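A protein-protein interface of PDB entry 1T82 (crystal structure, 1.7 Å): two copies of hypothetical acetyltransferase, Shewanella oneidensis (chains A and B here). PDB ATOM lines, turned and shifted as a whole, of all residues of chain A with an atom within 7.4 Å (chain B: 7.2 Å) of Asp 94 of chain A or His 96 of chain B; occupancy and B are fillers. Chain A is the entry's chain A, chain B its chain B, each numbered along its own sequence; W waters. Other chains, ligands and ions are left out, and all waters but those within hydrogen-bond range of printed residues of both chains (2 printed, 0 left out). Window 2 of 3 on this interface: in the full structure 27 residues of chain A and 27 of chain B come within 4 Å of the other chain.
Water W1 bridges the backbone carbonyl oxygen of Tyr 99 of chain B (3.0 Å) and the backbone carbonyl oxygen of Ala 93 of chain A (3.0 Å). Water W2 bridges O of Leu 92 of chain A and O of Tyr 99 of chain B.
Tyr 66 of chain A touches Ile 97 of chain B, and with the chains exchanged Ile 97 of chain A touches Tyr 66 of chain B. Asp 94 of chain A touches His 96 of chain B, but with the chains exchanged His 96 of chain A does not touch Asp 94 of chain B (4.3 Å). Asp 94 of chain A touches Ile 97 of chain B, and with the chains exchanged Ile 97 of chain A touches Asp 94 of chain B. Ala 95 of chain A touches His 96 of chain B, and with the chains exchanged His 96 of chain A touches Ala 95 of chain B. Of the 14 pairs that touch across the chains among the printed residues, 9 have their exchanged pair printed and touching as well.
Of the printed residues of chain B, Tyr 66 of chain A touches Tyr 66, Ile 97 and Tyr 99. Of the printed residues of chain B, Ala 93 of chain A touches Arg 98 and Tyr 99. Asp 94 of chain A touches just these residues of chain B: His 96 and Ile 97. Printed residues of chain B within 4 Å of His 96 of chain A: Ala 95. Printed residues of chain A within 4 Å of Ala 95 of chain B: His 96 (3.2 Å) and Ile 97 (2.9 Å). His 96 of chain B touches just these residues of chain A: Asp 94 (3.9 Å) and Ala 95 (3.1 Å). Printed residues of chain A within 4 Å of Ile 97 of chain B: Tyr 66, Asp 94 and Ala 95. The nearest printed residue of chain A that does not touch Tyr 99 of chain B is Asp 94 of chain A (4.3 Å).
CG of Tyr 66 of chain A touches CD2 of Tyr 66 of chain B, 3.3 Å away. Ile 97 of chain B touches Tyr 66 of chain A. Leu 92 of chain A touches Tyr 99 of chain B. Ala 93 of chain A touches Arg 98 of chain B. OD2 of Asp 94 of chain A touches CE1 of His 96 of chain B, 3.9 Å away. Asp 94 of chain A touches Ile 97 of chain B. Ile 97 of chain A touches Tyr 66 of chain B (CG2 to OH, 3.4 Å). O of Ile 97 of chain A touches CA of Asp 94 of chain B, 3.2 Å away.
Of the 14 printed residues of chain B, 7 touch a printed residue of chain A. Printed residues of chain B that touch a printed residue of chain A: Tyr 66, Asp 94, Ala 95, His 96, Ile 97, Arg 98 and Tyr 99. Printed residues of chain A that touch a printed residue of chain B: Tyr 66, Leu 92, Ala 93, Asp 94, Ala 95, His 96 and Ile 97. Among the printed residues, 14 pairs touch across the chains. Among the printed residues, no Asp or Glu carboxylate lies within 4 Å of a Lys or Arg side-chain nitrogen of the other chain.
The side-chain hydroxyl of Tyr 99 of chain B is in hydrogen-bond range of the side-chain hydroxyl of Tyr 66 of chain A (2.8 Å). ND1 of His 96 of chain A sits at hydrogen-bond distance from O of Ala 95 of chain B. The backbone NH (N) of Ile 97 of chain A lies within hydrogen-bond range of the backbone carbonyl oxygen (O) of Ala 95 of chain B (2.9 Å). A ring nitrogen (ND1) of His 96 of chain B is in hydrogen-bond range of the backbone carbonyl oxygen (O) of Ala 95 of chain A, at 3.1 Å. The backbone NH (N) of Tyr 99 of chain B is in hydrogen-bond range of the backbone carbonyl oxygen (O) of Ala 93 of chain A. The backbone carbonyl oxygen of Ala 95 of chain A lies within hydrogen-bond range of the backbone NH of Ile 97 of chain B (2.9 Å).
A ring nitrogen (NE2) of His 96 of chain B lies within hydrogen-bond range of the guanidinium group of Arg 98 of chain B (3.3 Å). The backbone NH (N) of Arg 98 of chain B sits at hydrogen-bond distance from the backbone carbonyl oxygen (O) of Gln 144 of chain B (2.9 Å). The backbone NH (N) of Leu 148 of chain B is in hydrogen-bond range of the backbone carbonyl oxygen (O) of Asp 94 of chain B (2.9 Å). O of Asp 94 of chain A lies within hydrogen-bond range of N of Leu 148 of chain A. The backbone NH (N) of His 96 of chain B is in hydrogen-bond range of the backbone carbonyl oxygen (O) of Asp 146 of chain B, at 2.9 Å. The backbone NH (N) of Ala 93 of chain A sits at hydrogen-bond distance from the backbone carbonyl oxygen (O) of Leu 148 of chain A (2.8 Å).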
ATOM      1  N   TYR A  66     -22.347  18.398 -31.811  1.00  0.00           N
ATOM      2  CA  TYR A  66     -21.799  17.086 -32.146  1.00  0.00           C
ATOM      3  C   TYR A  66     -21.403  17.003 -33.610  1.00  0.00           C
ATOM      4  O   TYR A  66     -20.318  16.529 -33.945  1.00  0.00           O
ATOM      5  CB  TYR A  66     -22.820  15.980 -31.886  1.00  0.00           C
ATOM      6  CG  TYR A  66     -22.312  14.598 -32.260  1.00  0.00           C
ATOM      7  CD1 TYR A  66     -21.586  13.838 -31.350  1.00  0.00           C
ATOM      8  CD2 TYR A  66     -22.549  14.060 -33.531  1.00  0.00           C
ATOM      9  CE1 TYR A  66     -21.110  12.571 -31.684  1.00  0.00           C
ATOM     10  CE2 TYR A  66     -22.072  12.789 -33.877  1.00  0.00           C
ATOM     11  CZ  TYR A  66     -21.354  12.052 -32.939  1.00  0.00           C
ATOM     12  OH  TYR A  66     -20.890  10.793 -33.256  1.00  0.00           O
ATOM     13  N   VAL A  91     -14.737   6.723 -41.935  1.00  0.00           N
ATOM     14  CA  VAL A  91     -15.890   6.322 -41.141  1.00  0.00           C
ATOM     15  C   VAL A  91     -15.705   6.518 -39.636  1.00  0.00           C
ATOM     16  O   VAL A  91     -14.666   6.165 -39.074  1.00  0.00           O
ATOM     17  CB  VAL A  91     -16.240   4.835 -41.416  1.00  0.00           C
ATOM     18  CG1 VAL A  91     -17.519   4.454 -40.693  1.00  0.00           C
ATOM     19  CG2 VAL A  91     -16.387   4.605 -42.915  1.00  0.00           C
ATOM     20  N   LEU A  92     -16.712   7.099 -38.988  1.00  0.00           N
ATOM     21  CA  LEU A  92     -16.669   7.309 -37.539  1.00  0.00           C
ATOM     22  C   LEU A  92     -17.256   6.048 -36.900  1.00  0.00           C
ATOM     23  O   LEU A  92     -18.442   5.760 -37.063  1.00  0.00           O
ATOM     24  CB  LEU A  92     -17.505   8.538 -37.150  1.00  0.00           C
ATOM     25  CG  LEU A  92     -17.594   8.870 -35.653  1.00  0.00           C
ATOM     26  CD1 LEU A  92     -16.198   9.101 -35.079  1.00  0.00           C
ATOM     27  CD2 LEU A  92     -18.455  10.111 -35.462  1.00  0.00           C
ATOM     28  N   ALA A  93     -16.422   5.293 -36.188  1.00  0.00           N
ATOM     29  CA  ALA A  93     -16.866   4.051 -35.556  1.00  0.00           C
ATOM     30  C   ALA A  93     -17.628   4.274 -34.253  1.00  0.00           C
ATOM     31  O   ALA A  93     -18.616   3.593 -33.973  1.00  0.00           O
ATOM     32  CB  ALA A  93     -15.669   3.146 -35.310  1.00  0.00           C
ATOM     33  N   ASP A  94     -17.152   5.213 -33.452  1.00  0.00           N
ATOM     34  CA  ASP A  94     -17.799   5.529 -32.192  1.00  0.00           C
ATOM     35  C   ASP A  94     -17.273   6.854 -31.691  1.00  0.00           C
ATOM     36  O   ASP A  94     -16.214   7.324 -32.118  1.00  0.00           O
ATOM     37  CB  ASP A  94     -17.535   4.444 -31.147  1.00  0.00           C
ATOM     38  CG  ASP A  94     -16.088   4.382 -30.728  1.00  0.00           C
ATOM     39  OD1 ASP A  94     -15.276   3.780 -31.466  1.00  0.00           O
ATOM     40  OD2 ASP A  94     -15.758   4.942 -29.659  1.00  0.00           O
ATOM     41  N   ALA A  95     -18.014   7.459 -30.776  1.00  0.00           N
ATOM     42  CA  ALA A  95     -17.610   8.740 -30.240  1.00  0.00           C
ATOM     43  C   ALA A  95     -18.196   8.975 -28.865  1.00  0.00           C
ATOM     44  O   ALA A  95     -19.251   8.446 -28.518  1.00  0.00           O
ATOM     45  CB  ALA A  95     -18.047   9.855 -31.188  1.00  0.00           C
ATOM     46  N   HIS A  96     -17.481   9.776 -28.090  1.00  0.00           N
ATOM     47  CA  HIS A  96     -17.894  10.153 -26.754  1.00  0.00           C
ATOM     48  C   HIS A  96     -17.861  11.675 -26.750  1.00  0.00           C
ATOM     49  O   HIS A  96     -16.886  12.270 -27.199  1.00  0.00           O
ATOM     50  CB  HIS A  96     -16.915   9.601 -25.714  1.00  0.00           C
ATOM     51  CG  HIS A  96     -17.176  10.087 -24.323  1.00  0.00           C
ATOM     52  ND1 HIS A  96     -18.434  10.089 -23.759  1.00  0.00           N
ATOM     53  CD2 HIS A  96     -16.343  10.593 -23.382  1.00  0.00           C
ATOM     54  CE1 HIS A  96     -18.366  10.576 -22.533  1.00  0.00           C
ATOM     55  NE2 HIS A  96     -17.108  10.890 -22.280  1.00  0.00           N
ATOM     56  N   ILE A  97     -18.929  12.305 -26.271  1.00  0.00           N
ATOM     57  CA  ILE A  97     -18.983  13.759 -26.227  1.00  0.00           C
ATOM     58  C   ILE A  97     -19.479  14.232 -24.870  1.00  0.00           C
ATOM     59  O   ILE A  97     -20.398  13.647 -24.287  1.00  0.00           O
ATOM     60  CB  ILE A  97     -19.889  14.333 -27.366  1.00  0.00           C
ATOM     61  CG1 ILE A  97     -19.917  15.866 -27.304  1.00  0.00           C
ATOM     62  CG2 ILE A  97     -21.305  13.779 -27.248  1.00  0.00           C
ATOM     63  CD1 ILE A  97     -20.554  16.530 -28.538  1.00  0.00           C
ATOM     64  N   LYS A 130      -7.608   7.828 -33.252  1.00  0.00           N
ATOM     65  CA  LYS A 130      -8.481   8.356 -32.215  1.00  0.00           C
ATOM     66  C   LYS A 130      -8.215   9.853 -32.174  1.00  0.00           C
ATOM     67  O   LYS A 130      -7.091  10.284 -31.905  1.00  0.00           O
ATOM     68  CB  LYS A 130      -8.155   7.722 -30.860  1.00  0.00           C
ATOM     69  CG  LYS A 130      -9.084   8.155 -29.727  1.00  0.00           C
ATOM     70  CD  LYS A 130      -8.825   7.352 -28.454  1.00  0.00           C
ATOM     71  CE  LYS A 130      -9.771   7.756 -27.331  1.00  0.00           C
ATOM     72  NZ  LYS A 130     -11.199   7.518 -27.676  1.00  0.00           N
ATOM     73  N   PHE A 145     -14.865  16.155 -27.357  1.00  0.00           N
ATOM     74  CA  PHE A 145     -15.269  15.048 -28.219  1.00  0.00           C
ATOM     75  C   PHE A 145     -14.104  14.106 -28.487  1.00  0.00           C
ATOM     76  O   PHE A 145     -12.987  14.546 -28.747  1.00  0.00           O
ATOM     77  CB  PHE A 145     -15.808  15.638 -29.532  1.00  0.00           C
ATOM     78  CG  PHE A 145     -16.053  14.634 -30.638  1.00  0.00           C
ATOM     79  CD1 PHE A 145     -14.997  14.124 -31.395  1.00  0.00           C
ATOM     80  CD2 PHE A 145     -17.352  14.282 -30.989  1.00  0.00           C
ATOM     81  CE1 PHE A 145     -15.237  13.281 -32.492  1.00  0.00           C
ATOM     82  CE2 PHE A 145     -17.604  13.446 -32.080  1.00  0.00           C
ATOM     83  CZ  PHE A 145     -16.546  12.946 -32.834  1.00  0.00           C
ATOM     84  N   ASP A 146     -14.366  12.808 -28.399  1.00  0.00           N
ATOM     85  CA  ASP A 146     -13.345  11.809 -28.670  1.00  0.00           C
ATOM     86  C   ASP A 146     -13.946  10.815 -29.648  1.00  0.00           C
ATOM     87  O   ASP A 146     -14.913  10.121 -29.332  1.00  0.00           O
ATOM     88  CB  ASP A 146     -12.920  11.122 -27.374  1.00  0.00           C
ATOM     89  CG  ASP A 146     -12.101  12.037 -26.485  1.00  0.00           C
ATOM     90  OD1 ASP A 146     -10.930  12.302 -26.832  1.00  0.00           O
ATOM     91  OD2 ASP A 146     -12.631  12.502 -25.454  1.00  0.00           O
ATOM     92  N   GLY A 147     -13.384  10.761 -30.849  1.00  0.00           N
ATOM     93  CA  GLY A 147     -13.922   9.858 -31.845  1.00  0.00           C
ATOM     94  C   GLY A 147     -12.908   8.937 -32.480  1.00  0.00           C
ATOM     95  O   GLY A 147     -11.740   9.294 -32.650  1.00  0.00           O
ATOM     96  N   LEU A 148     -13.361   7.738 -32.821  1.00  0.00           N
ATOM     97  CA  LEU A 148     -12.509   6.758 -33.470  1.00  0.00           C
ATOM     98  C   LEU A 148     -12.843   6.768 -34.954  1.00  0.00           C
ATOM     99  O   LEU A 148     -13.928   6.346 -35.362  1.00  0.00           O
ATOM    100  CB  LEU A 148     -12.746   5.359 -32.897  1.00  0.00           C
ATOM    101  CG  LEU A 148     -11.872   4.267 -33.520  1.00  0.00           C
ATOM    102  CD1 LEU A 148     -10.405   4.549 -33.225  1.00  0.00           C
ATOM    103  CD2 LEU A 148     -12.272   2.905 -32.966  1.00  0.00           C
ATOM    104  N   TYR A 149     -11.910   7.272 -35.755  1.00  0.00           N
ATOM    105  CA  TYR A 149     -12.093   7.336 -37.199  1.00  0.00           C
ATOM    106  C   TYR A 149     -11.266   6.275 -37.888  1.00  0.00           C
ATOM    107  O   TYR A 149     -10.109   6.058 -37.543  1.00  0.00           O
ATOM    108  CB  TYR A 149     -11.667   8.693 -37.749  1.00  0.00           C
ATOM    109  CG  TYR A 149     -12.528   9.839 -37.294  1.00  0.00           C
ATOM    110  CD1 TYR A 149     -12.329  10.430 -36.048  1.00  0.00           C
ATOM    111  CD2 TYR A 149     -13.539  10.341 -38.118  1.00  0.00           C
ATOM    112  CE1 TYR A 149     -13.109  11.499 -35.633  1.00  0.00           C
ATOM    113  CE2 TYR A 149     -14.330  11.407 -37.711  1.00  0.00           C
ATOM    114  CZ  TYR A 149     -14.104  11.982 -36.466  1.00  0.00           C
ATOM    115  OH  TYR A 149     -14.863  13.046 -36.051  1.00  0.00           O
ATOM    116  N   VAL A 150     -11.859   5.632 -38.880  1.00  0.00           N
ATOM    117  CA  VAL A 150     -11.161   4.600 -39.620  1.00  0.00           C
ATOM    118  C   VAL A 150     -11.129   4.964 -41.098  1.00  0.00           C
ATOM    119  O   VAL A 150     -12.138   5.384 -41.664  1.00  0.00           O
ATOM    120  CB  VAL A 150     -11.861   3.237 -39.452  1.00  0.00           C
ATOM    121  CG1 VAL A 150     -11.069   2.154 -40.163  1.00  0.00           C
ATOM    122  CG2 VAL A 150     -12.004   2.910 -37.967  1.00  0.00           C
ATOM    123  N   TYR B  66     -26.763  10.681 -34.877  1.00  0.00           N
ATOM    124  CA  TYR B  66     -26.594  11.153 -33.507  1.00  0.00           C
ATOM    125  C   TYR B  66     -27.689  12.133 -33.108  1.00  0.00           C
ATOM    126  O   TYR B  66     -28.286  12.027 -32.031  1.00  0.00           O
ATOM    127  CB  TYR B  66     -25.248  11.855 -33.334  1.00  0.00           C
ATOM    128  CG  TYR B  66     -25.057  12.456 -31.955  1.00  0.00           C
ATOM    129  CD1 TYR B  66     -24.488  11.713 -30.917  1.00  0.00           C
ATOM    130  CD2 TYR B  66     -25.459  13.770 -31.684  1.00  0.00           C
ATOM    131  CE1 TYR B  66     -24.317  12.267 -29.650  1.00  0.00           C
ATOM    132  CE2 TYR B  66     -25.296  14.324 -30.415  1.00  0.00           C
ATOM    133  CZ  TYR B  66     -24.723  13.569 -29.410  1.00  0.00           C
ATOM    134  OH  TYR B  66     -24.533  14.119 -28.165  1.00  0.00           O
ATOM    135  N   LEU B  92     -28.455  17.756 -22.362  1.00  0.00           N
ATOM    136  CA  LEU B  92     -27.625  16.563 -22.464  1.00  0.00           C
ATOM    137  C   LEU B  92     -26.243  16.904 -21.915  1.00  0.00           C
ATOM    138  O   LEU B  92     -25.599  17.854 -22.369  1.00  0.00           O
ATOM    139  CB  LEU B  92     -27.517  16.108 -23.923  1.00  0.00           C
ATOM    140  CG  LEU B  92     -26.631  14.893 -24.224  1.00  0.00           C
ATOM    141  CD1 LEU B  92     -27.166  13.641 -23.529  1.00  0.00           C
ATOM    142  CD2 LEU B  92     -26.594  14.683 -25.729  1.00  0.00           C
ATOM    143  N   ASP B  94     -23.616  14.319 -21.260  1.00  0.00           N
ATOM    144  CA  ASP B  94     -22.610  13.497 -21.913  1.00  0.00           C
ATOM    145  C   ASP B  94     -23.280  12.354 -22.644  1.00  0.00           C
ATOM    146  O   ASP B  94     -24.354  11.888 -22.257  1.00  0.00           O
ATOM    147  CB  ASP B  94     -21.608  12.951 -20.893  1.00  0.00           C
ATOM    148  CG  ASP B  94     -22.268  12.150 -19.798  1.00  0.00           C
ATOM    149  OD1 ASP B  94     -22.992  12.749 -18.971  1.00  0.00           O
ATOM    150  OD2 ASP B  94     -22.067  10.916 -19.761  1.00  0.00           O
ATOM    151  N   ALA B  95     -22.643  11.901 -23.711  1.00  0.00           N
ATOM    152  CA  ALA B  95     -23.209  10.821 -24.482  1.00  0.00           C
ATOM    153  C   ALA B  95     -22.142  10.012 -25.181  1.00  0.00           C
ATOM    154  O   ALA B  95     -21.052  10.504 -25.470  1.00  0.00           O
ATOM    155  CB  ALA B  95     -24.193  11.377 -25.499  1.00  0.00           C
ATOM    156  N   HIS B  96     -22.474   8.755 -25.433  1.00  0.00           N
ATOM    157  CA  HIS B  96     -21.589   7.839 -26.125  1.00  0.00           C
ATOM    158  C   HIS B  96     -22.409   7.207 -27.237  1.00  0.00           C
ATOM    159  O   HIS B  96     -23.542   6.783 -27.015  1.00  0.00           O
ATOM    160  CB  HIS B  96     -21.089   6.761 -25.166  1.00  0.00           C
ATOM    161  CG  HIS B  96     -20.248   5.716 -25.825  1.00  0.00           C
ATOM    162  ND1 HIS B  96     -19.172   6.027 -26.626  1.00  0.00           N
ATOM    163  CD2 HIS B  96     -20.323   4.364 -25.802  1.00  0.00           C
ATOM    164  CE1 HIS B  96     -18.620   4.912 -27.070  1.00  0.00           C
ATOM    165  NE2 HIS B  96     -19.299   3.889 -26.584  1.00  0.00           N
ATOM    166  N   ILE B  97     -21.847   7.150 -28.439  1.00  0.00           N
ATOM    167  CA  ILE B  97     -22.565   6.554 -29.562  1.00  0.00           C
ATOM    168  C   ILE B  97     -21.663   5.596 -30.326  1.00  0.00           C
ATOM    169  O   ILE B  97     -20.478   5.865 -30.521  1.00  0.00           O
ATOM    170  CB  ILE B  97     -23.110   7.648 -30.530  1.00  0.00           C
ATOM    171  CG1 ILE B  97     -23.907   7.000 -31.668  1.00  0.00           C
ATOM    172  CG2 ILE B  97     -21.957   8.472 -31.090  1.00  0.00           C
ATOM    173  CD1 ILE B  97     -24.724   7.987 -32.500  1.00  0.00           C
ATOM    174  N   ARG B  98     -22.225   4.460 -30.729  1.00  0.00           N
ATOM    175  CA  ARG B  98     -21.485   3.471 -31.497  1.00  0.00           C
ATOM    176  C   ARG B  98     -22.255   3.231 -32.785  1.00  0.00           C
ATOM    177  O   ARG B  98     -23.467   3.021 -32.761  1.00  0.00           O
ATOM    178  CB  ARG B  98     -21.359   2.154 -30.724  1.00  0.00           C
ATOM    179  CG  ARG B  98     -20.746   2.302 -29.340  1.00  0.00           C
ATOM    180  CD  ARG B  98     -20.481   0.943 -28.699  1.00  0.00           C
ATOM    181  NE  ARG B  98     -19.350   0.267 -29.324  1.00  0.00           N
ATOM    182  CZ  ARG B  98     -18.078   0.598 -29.125  1.00  0.00           C
ATOM    183  NH1 ARG B  98     -17.111  -0.072 -29.744  1.00  0.00           N
ATOM    184  NH2 ARG B  98     -17.767   1.585 -28.293  1.00  0.00           N
ATOM    185  N   TYR B  99     -21.551   3.283 -33.909  1.00  0.00           N
ATOM    186  CA  TYR B  99     -22.174   3.053 -35.203  1.00  0.00           C
ATOM    187  C   TYR B  99     -21.853   1.620 -35.612  1.00  0.00           C
ATOM    188  O   TYR B  99     -20.694   1.276 -35.844  1.00  0.00           O
ATOM    189  CB  TYR B  99     -21.633   4.045 -36.233  1.00  0.00           C
ATOM    190  CG  TYR B  99     -21.890   5.496 -35.880  1.00  0.00           C
ATOM    191  CD1 TYR B  99     -21.002   6.211 -35.075  1.00  0.00           C
ATOM    192  CD2 TYR B  99     -23.012   6.159 -36.371  1.00  0.00           C
ATOM    193  CE1 TYR B  99     -21.225   7.559 -34.776  1.00  0.00           C
ATOM    194  CE2 TYR B  99     -23.248   7.494 -36.075  1.00  0.00           C
ATOM    195  CZ  TYR B  99     -22.354   8.189 -35.285  1.00  0.00           C
ATOM    196  OH  TYR B  99     -22.584   9.513 -35.011  1.00  0.00           O
ATOM    197  N   VAL B 133     -30.745   4.821 -26.137  1.00  0.00           N
ATOM    198  CA  VAL B 133     -31.509   4.949 -27.366  1.00  0.00           C
ATOM    199  C   VAL B 133     -30.920   3.993 -28.390  1.00  0.00           C
ATOM    200  O   VAL B 133     -29.701   3.868 -28.494  1.00  0.00           O
ATOM    201  CB  VAL B 133     -31.439   6.389 -27.926  1.00  0.00           C
ATOM    202  CG1 VAL B 133     -32.295   6.498 -29.179  1.00  0.00           C
ATOM    203  CG2 VAL B 133     -31.906   7.388 -26.875  1.00  0.00           C
ATOM    204  N   GLN B 144     -26.088   2.510 -31.471  1.00  0.00           N
ATOM    205  CA  GLN B 144     -26.362   2.468 -30.033  1.00  0.00           C
ATOM    206  C   GLN B 144     -25.963   3.792 -29.385  1.00  0.00           C
ATOM    207  O   GLN B 144     -24.879   4.317 -29.639  1.00  0.00           O
ATOM    208  CB  GLN B 144     -25.576   1.322 -29.392  1.00  0.00           C
ATOM    209  CG  GLN B 144     -25.973   1.003 -27.965  1.00  0.00           C
ATOM    210  CD  GLN B 144     -27.396   0.482 -27.861  1.00  0.00           C
ATOM    211  OE1 GLN B 144     -27.726  -0.577 -28.401  1.00  0.00           O
ATOM    212  NE2 GLN B 144     -28.248   1.227 -27.171  1.00  0.00           N
ATOM    213  N   PHE B 145     -26.832   4.300 -28.519  1.00  0.00           N
ATOM    214  CA  PHE B 145     -26.616   5.582 -27.858  1.00  0.00           C
ATOM    215  C   PHE B 145     -26.895   5.528 -26.360  1.00  0.00           C
ATOM    216  O   PHE B 145     -27.871   4.932 -25.914  1.00  0.00           O
ATOM    217  CB  PHE B 145     -27.523   6.615 -28.542  1.00  0.00           C
ATOM    218  CG  PHE B 145     -27.526   7.982 -27.902  1.00  0.00           C
ATOM    219  CD1 PHE B 145     -28.340   8.258 -26.807  1.00  0.00           C
ATOM    220  CD2 PHE B 145     -26.782   9.019 -28.461  1.00  0.00           C
ATOM    221  CE1 PHE B 145     -28.424   9.553 -26.279  1.00  0.00           C
ATOM    222  CE2 PHE B 145     -26.856  10.311 -27.944  1.00  0.00           C
ATOM    223  CZ  PHE B 145     -27.681  10.579 -26.853  1.00  0.00           C
ATOM    224  N   ASP B 146     -26.008   6.144 -25.588  1.00  0.00           N
ATOM    225  CA  ASP B 146     -26.157   6.215 -24.147  1.00  0.00           C
ATOM    226  C   ASP B 146     -25.979   7.675 -23.783  1.00  0.00           C
ATOM    227  O   ASP B 146     -24.942   8.271 -24.065  1.00  0.00           O
ATOM    228  CB  ASP B 146     -25.109   5.340 -23.461  1.00  0.00           C
ATOM    229  CG  ASP B 146     -25.455   3.864 -23.542  1.00  0.00           C
ATOM    230  OD1 ASP B 146     -26.467   3.465 -22.928  1.00  0.00           O
ATOM    231  OD2 ASP B 146     -24.732   3.109 -24.224  1.00  0.00           O
ATOM    232  N   GLY B 147     -27.006   8.263 -23.183  1.00  0.00           N
ATOM    233  CA  GLY B 147     -26.915   9.660 -22.827  1.00  0.00           C
ATOM    234  C   GLY B 147     -27.342   9.972 -21.413  1.00  0.00           C
ATOM    235  O   GLY B 147     -28.264   9.364 -20.871  1.00  0.00           O
ATOM    236  N   LEU B 148     -26.645  10.917 -20.802  1.00  0.00           N
ATOM    237  CA  LEU B 148     -26.981  11.342 -19.453  1.00  0.00           C
ATOM    238  C   LEU B 148     -27.618  12.714 -19.593  1.00  0.00           C
ATOM    239  O   LEU B 148     -26.958  13.664 -20.010  1.00  0.00           O
ATOM    240  CB  LEU B 148     -25.723  11.441 -18.585  1.00  0.00           C
ATOM    241  CG  LEU B 148     -25.946  12.006 -17.177  1.00  0.00           C
ATOM    242  CD1 LEU B 148     -26.921  11.124 -16.420  1.00  0.00           C
ATOM    243  CD2 LEU B 148     -24.616  12.097 -16.440  1.00  0.00           C
HETATM  244  O   HOH W   1     -18.562   0.595 -33.919  1.00  0.00           O
HETATM  245  O   HOH W   2     -19.340   2.858 -38.589  1.00  0.00           O
